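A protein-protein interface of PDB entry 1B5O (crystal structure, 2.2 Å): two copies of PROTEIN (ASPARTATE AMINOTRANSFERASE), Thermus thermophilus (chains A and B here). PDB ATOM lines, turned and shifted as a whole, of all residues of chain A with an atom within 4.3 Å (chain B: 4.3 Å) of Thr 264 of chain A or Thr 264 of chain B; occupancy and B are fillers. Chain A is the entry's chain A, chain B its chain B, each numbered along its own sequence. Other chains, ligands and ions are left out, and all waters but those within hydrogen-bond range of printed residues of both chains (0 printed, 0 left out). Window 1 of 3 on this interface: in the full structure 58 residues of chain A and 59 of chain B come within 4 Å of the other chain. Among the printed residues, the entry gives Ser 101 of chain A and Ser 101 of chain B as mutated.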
ATOM      1  N   VAL A  98       9.317 -14.079  12.261  1.00  0.00           N
ATOM      2  CA  VAL A  98      10.525 -13.432  12.771  1.00  0.00           C
ATOM      3  C   VAL A  98      10.031 -12.273  13.636  1.00  0.00           C
ATOM      4  O   VAL A  98       9.911 -11.132  13.179  1.00  0.00           O
ATOM      5  CB  VAL A  98      11.432 -12.913  11.617  1.00  0.00           C
ATOM      6  CG1 VAL A  98      12.690 -12.267  12.184  1.00  0.00           C
ATOM      7  CG2 VAL A  98      11.818 -14.061  10.691  1.00  0.00           C
ATOM      8  N   SER A 101       6.499  -8.672  15.198  1.00  0.00           N
ATOM      9  CA  SER A 101       6.436  -7.589  14.226  1.00  0.00           C
ATOM     10  C   SER A 101       6.257  -8.124  12.803  1.00  0.00           C
ATOM     11  O   SER A 101       5.549  -7.514  12.000  1.00  0.00           O
ATOM     12  CB  SER A 101       7.672  -6.689  14.317  1.00  0.00           C
ATOM     13  OG  SER A 101       8.854  -7.399  13.980  1.00  0.00           O
ATOM     14  N   GLN A 102       6.865  -9.274  12.495  1.00  0.00           N
ATOM     15  CA  GLN A 102       6.736  -9.840  11.152  1.00  0.00           C
ATOM     16  C   GLN A 102       5.352 -10.429  10.942  1.00  0.00           C
ATOM     17  O   GLN A 102       4.837 -10.419   9.828  1.00  0.00           O
ATOM     18  CB  GLN A 102       7.797 -10.904  10.847  1.00  0.00           C
ATOM     19  CG  GLN A 102       8.001 -11.042   9.346  1.00  0.00           C
ATOM     20  CD  GLN A 102       8.483 -12.402   8.898  1.00  0.00           C
ATOM     21  OE1 GLN A 102       8.467 -13.367   9.649  1.00  0.00           O
ATOM     22  NE2 GLN A 102       8.896 -12.483   7.643  1.00  0.00           N
ATOM     23  N   ARG A 242      14.103 -13.034  17.980  1.00  0.00           N
ATOM     24  CA  ARG A 242      13.218 -12.789  16.839  1.00  0.00           C
ATOM     25  C   ARG A 242      12.263 -13.952  16.481  1.00  0.00           C
ATOM     26  O   ARG A 242      12.326 -14.522  15.387  1.00  0.00           O
ATOM     27  CB  ARG A 242      14.030 -12.353  15.612  1.00  0.00           C
ATOM     28  CG  ARG A 242      15.064 -11.221  15.857  1.00  0.00           C
ATOM     29  CD  ARG A 242      14.467  -9.950  16.509  1.00  0.00           C
ATOM     30  NE  ARG A 242      13.353  -9.376  15.752  1.00  0.00           N
ATOM     31  CZ  ARG A 242      12.155  -9.117  16.276  1.00  0.00           C
ATOM     32  NH1 ARG A 242      11.921  -9.367  17.554  1.00  0.00           N
ATOM     33  NH2 ARG A 242      11.172  -8.668  15.513  1.00  0.00           N
ATOM     34  N   SER A 260       6.223 -15.170   3.733  1.00  0.00           N
ATOM     35  CA  SER A 260       7.468 -15.550   4.401  1.00  0.00           C
ATOM     36  C   SER A 260       8.422 -16.255   3.440  1.00  0.00           C
ATOM     37  O   SER A 260       9.602 -15.914   3.381  1.00  0.00           O
ATOM     38  CB  SER A 260       7.196 -16.480   5.584  1.00  0.00           C
ATOM     39  OG  SER A 260       6.632 -15.767   6.667  1.00  0.00           O
ATOM     40  N   SER A 263      10.279 -13.877   1.340  1.00  0.00           N
ATOM     41  CA  SER A 263      11.048 -12.832   2.004  1.00  0.00           C
ATOM     42  C   SER A 263      12.154 -13.297   2.945  1.00  0.00           C
ATOM     43  O   SER A 263      13.332 -13.079   2.671  1.00  0.00           O
ATOM     44  CB  SER A 263      10.095 -11.863   2.727  1.00  0.00           C
ATOM     45  OG  SER A 263       9.172 -12.562   3.545  1.00  0.00           O
ATOM     46  N   THR A 264      11.771 -13.937   4.044  1.00  0.00           N
ATOM     47  CA  THR A 264      12.719 -14.399   5.045  1.00  0.00           C
ATOM     48  C   THR A 264      12.954 -15.898   4.974  1.00  0.00           C
ATOM     49  O   THR A 264      13.865 -16.418   5.636  1.00  0.00           O
ATOM     50  CB  THR A 264      12.210 -14.062   6.466  1.00  0.00           C
ATOM     51  OG1 THR A 264      10.867 -14.542   6.617  1.00  0.00           O
ATOM     52  CG2 THR A 264      12.234 -12.549   6.723  1.00  0.00           C
ATOM     53  N   THR A 265      12.132 -16.574   4.166  1.00  0.00           N
ATOM     54  CA  THR A 265      12.159 -18.031   3.971  1.00  0.00           C
ATOM     55  C   THR A 265      11.573 -18.738   5.194  1.00  0.00           C
ATOM     56  O   THR A 265      10.554 -19.403   5.095  1.00  0.00           O
ATOM     57  CB  THR A 265      13.583 -18.561   3.670  1.00  0.00           C
ATOM     58  OG1 THR A 265      14.109 -17.873   2.532  1.00  0.00           O
ATOM     59  CG2 THR A 265      13.558 -20.057   3.381  1.00  0.00           C
ATOM     60  N   SER A 266      12.215 -18.566   6.345  1.00  0.00           N
ATOM     61  CA  SER A 266      11.763 -19.156   7.604  1.00  0.00           C
ATOM     62  C   SER A 266      12.592 -18.547   8.737  1.00  0.00           C
ATOM     63  O   SER A 266      13.710 -18.087   8.504  1.00  0.00           O
ATOM     64  CB  SER A 266      11.963 -20.677   7.589  1.00  0.00           C
ATOM     65  OG  SER A 266      11.437 -21.279   8.770  1.00  0.00           O
ATOM     66  N   VAL B  98      17.843 -10.920   7.270  1.00  0.00           N
ATOM     67  CA  VAL B  98      17.405 -12.272   7.620  1.00  0.00           C
ATOM     68  C   VAL B  98      17.590 -13.109   6.357  1.00  0.00           C
ATOM     69  O   VAL B  98      16.651 -13.357   5.588  1.00  0.00           O
ATOM     70  CB  VAL B  98      15.922 -12.294   8.125  1.00  0.00           C
ATOM     71  CG1 VAL B  98      15.478 -13.716   8.495  1.00  0.00           C
ATOM     72  CG2 VAL B  98      15.778 -11.391   9.347  1.00  0.00           C
ATOM     73  N   SER B 101      17.925 -13.742   1.160  1.00  0.00           N
ATOM     74  CA  SER B 101      16.600 -13.625   0.570  1.00  0.00           C
ATOM     75  C   SER B 101      15.919 -12.326   1.039  1.00  0.00           C
ATOM     76  O   SER B 101      15.259 -11.652   0.246  1.00  0.00           O
ATOM     77  CB  SER B 101      15.747 -14.866   0.872  1.00  0.00           C
ATOM     78  OG  SER B 101      15.557 -15.057   2.270  1.00  0.00           O
ATOM     79  N   GLN B 102      16.121 -11.927   2.296  1.00  0.00           N
ATOM     80  CA  GLN B 102      15.494 -10.688   2.756  1.00  0.00           C
ATOM     81  C   GLN B 102      16.173  -9.437   2.213  1.00  0.00           C
ATOM     82  O   GLN B 102      15.549  -8.381   2.143  1.00  0.00           O
ATOM     83  CB  GLN B 102      15.370 -10.593   4.271  1.00  0.00           C
ATOM     84  CG  GLN B 102      14.523  -9.376   4.665  1.00  0.00           C
ATOM     85  CD  GLN B 102      14.630  -8.986   6.129  1.00  0.00           C
ATOM     86  OE1 GLN B 102      15.689  -9.098   6.740  1.00  0.00           O
ATOM     87  NE2 GLN B 102      13.529  -8.495   6.687  1.00  0.00           N
ATOM     88  N   ARG B 242      19.858 -17.985   9.123  1.00  0.00           N
ATOM     89  CA  ARG B 242      19.205 -16.841   8.478  1.00  0.00           C
ATOM     90  C   ARG B 242      19.952 -15.505   8.611  1.00  0.00           C
ATOM     91  O   ARG B 242      19.423 -14.533   9.169  1.00  0.00           O
ATOM     92  CB  ARG B 242      17.758 -16.667   8.979  1.00  0.00           C
ATOM     93  CG  ARG B 242      16.901 -17.937   9.078  1.00  0.00           C
ATOM     94  CD  ARG B 242      16.754 -18.685   7.764  1.00  0.00           C
ATOM     95  NE  ARG B 242      16.359 -17.811   6.667  1.00  0.00           N
ATOM     96  CZ  ARG B 242      17.040 -17.707   5.528  1.00  0.00           C
ATOM     97  NH1 ARG B 242      18.139 -18.427   5.349  1.00  0.00           N
ATOM     98  NH2 ARG B 242      16.653 -16.850   4.590  1.00  0.00           N
ATOM     99  N   SER B 260      13.388  -3.077   6.993  1.00  0.00           N
ATOM    100  CA  SER B 260      13.600  -4.051   8.060  1.00  0.00           C
ATOM    101  C   SER B 260      12.990  -3.547   9.371  1.00  0.00           C
ATOM    102  O   SER B 260      12.382  -4.320  10.104  1.00  0.00           O
ATOM    103  CB  SER B 260      15.093  -4.341   8.276  1.00  0.00           C
ATOM    104  OG  SER B 260      15.694  -4.965   7.151  1.00  0.00           O
ATOM    105  N   SER B 263       9.356  -4.335   9.560  1.00  0.00           N
ATOM    106  CA  SER B 263       8.990  -5.735   9.363  1.00  0.00           C
ATOM    107  C   SER B 263       9.598  -6.733  10.340  1.00  0.00           C
ATOM    108  O   SER B 263       8.887  -7.311  11.157  1.00  0.00           O
ATOM    109  CB  SER B 263       9.286  -6.164   7.916  1.00  0.00           C
ATOM    110  OG  SER B 263      10.632  -5.892   7.554  1.00  0.00           O
ATOM    111  N   THR B 264      10.907  -6.946  10.247  1.00  0.00           N
ATOM    112  CA  THR B 264      11.574  -7.907  11.115  1.00  0.00           C
ATOM    113  C   THR B 264      12.287  -7.262  12.296  1.00  0.00           C
ATOM    114  O   THR B 264      12.696  -7.961  13.230  1.00  0.00           O
ATOM    115  CB  THR B 264      12.612  -8.733  10.322  1.00  0.00           C
ATOM    116  OG1 THR B 264      13.471  -7.843   9.599  1.00  0.00           O
ATOM    117  CG2 THR B 264      11.929  -9.673   9.346  1.00  0.00           C
ATOM    118  N   THR B 265      12.407  -5.935  12.247  1.00  0.00           N
ATOM    119  CA  THR B 265      13.098  -5.119  13.257  1.00  0.00           C
ATOM    120  C   THR B 265      14.607  -5.261  13.073  1.00  0.00           C
ATOM    121  O   THR B 265      15.285  -4.295  12.741  1.00  0.00           O
ATOM    122  CB  THR B 265      12.699  -5.482  14.701  1.00  0.00           C
ATOM    123  OG1 THR B 265      11.288  -5.304  14.858  1.00  0.00           O
ATOM    124  CG2 THR B 265      13.420  -4.584  15.704  1.00  0.00           C
ATOM    125  N   SER B 266      15.109  -6.480  13.251  1.00  0.00           N
ATOM    126  CA  SER B 266      16.531  -6.789  13.096  1.00  0.00           C
ATOM    127  C   SER B 266      16.724  -8.303  13.175  1.00  0.00           C
ATOM    128  O   SER B 266      15.894  -9.002  13.752  1.00  0.00           O
ATOM    129  CB  SER B 266      17.346  -6.133  14.212  1.00  0.00           C
ATOM    130  OG  SER B 266      18.734  -6.313  13.982  1.00  0.00           O
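Thr 264 of chain A touches just these residues of chain B: Val 98, Ser 101, Arg 242 and Thr 264.
Thr 264 of chain B touches just these residues of chain A: Val 98 (3.9 Å), Ser 101 (3.8 Å), Arg 242 (2.8 Å) and Thr 264 (3.9 Å).
Printed residues of chain B within 4 Å of Thr 265 of chain A: Ser 101 and Arg 242.
Of the printed residues of chain B, Gln 102 of chain A touches Ser 263.
Printed residues of chain B within 4 Å of Ser 266 of chain A: Arg 242 (3.2 Å).
The nearest residue of chain A that does not touch Thr 264 of chain B is Gln 102 of chain A (4.2 Å).
Among the printed residues, merely in contact across the chains: Val 98 of chain A with Thr 264 of chain B (3.9 Å), Ser 101 of chain A with Thr 264 of chain B (3.8 Å), Thr 264 of chain A with Val 98 of chain B (3.9 Å), Thr 264 of chain A with Ser 101 of chain B (3.8 Å) and Thr 264 of chain A with Thr 264 of chain B (3.9 Å).
The backbone NH (N) of Val 98 of chain A lies within hydrogen-bond range of the side-chain amide oxygen (OE1) of Gln 102 of chain A, 2.8 Å away.
The guanidinium group of Arg 242 of chain A is in hydrogen-bond range of the side-chain hydroxyl of Ser 101 of chain A.
The backbone NH of Val 98 of chain B sits at hydrogen-bond distance from the side-chain amide oxygen of Gln 102 of chain B.
The side-chain hydroxyl (OG) of Ser 101 of chain B is in hydrogen-bond range of the guanidinium group (NH2) of Arg 242 of chain B (3.1 Å).
OG1 of Thr 264 of chain B is in hydrogen-bond range of NE2 of Gln 102 of chain B (3.0 Å).
The backbone carbonyl oxygen of Ser 260 of chain B is in hydrogen-bond range of the side-chain hydroxyl of Ser 263 of chain B (3.5 Å).
Val 98 of chain A touches Thr 264 of chain B, and with the chains exchanged Thr 264 of chain A touches Val 98 of chain B.
Ser 101 of chain A touches Ser 263 of chain B, and with the chains exchanged Ser 263 of chain A touches Ser 101 of chain B.
Ser 101 of chain A touches Thr 265 of chain B, and with the chains exchanged Thr 265 of chain A touches Ser 101 of chain B.
Thr 264 of chain B touches its own counterpart, Thr 264 of chain A.
9 positions are printed for both chains.
OG of Ser 101 of chain A sits at hydrogen-bond distance from O of Ser 263 of chain B (2.8 Å).
OG1 of Thr 265 of chain B is in hydrogen-bond range of OG of Ser 101 of chain A (3.3 Å).
The backbone carbonyl oxygen (O) of Ser 263 of chain B lies within hydrogen-bond range of the backbone NH (N) of Gln 102 of chain A, at 3.1 Å.
The guanidinium group of Arg 242 of chain A sits at hydrogen-bond distance from the backbone carbonyl oxygen of Thr 264 of chain B.
The guanidinium group (NH2) of Arg 242 of chain A lies within hydrogen-bond range of the side-chain hydroxyl (OG1) of Thr 265 of chain B, 3.4 Å away.
The backbone carbonyl oxygen (O) of Ser 266 of chain B sits close to the guanidinium group (NE) of Arg 242 of chain A, at 3.3 Å.
O of Ser 263 of chain A lies within hydrogen-bond range of OG of Ser 101 of chain B (3.0 Å).
O of Ser 263 of chain A sits at hydrogen-bond distance from N of Gln 102 of chain B, 3.0 Å away.
The guanidinium group (NH2) of Arg 242 of chain B lies within hydrogen-bond range of the backbone carbonyl oxygen (O) of Thr 264 of chain A.
OG of Ser 101 of chain B is in hydrogen-bond range of OG1 of Thr 265 of chain A, at 3.2 Å.
The guanidinium group of Arg 242 of chain B lies within hydrogen-bond range of the side-chain hydroxyl of Thr 265 of chain A (3.4 Å).
The backbone carbonyl oxygen (O) of Ser 266 of chain A sits close to the guanidinium group (NE) of Arg 242 of chain B, 3.2 Å away.
Hydrophobic or aromatic side chains of chain A that line the printed part of chain B: Val 98.
Hydrophobic or aromatic side chains of chain B within 4 Å of the printed part of chain A: Val 98.
Among the printed residues, 17 pairs touch across the chains.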
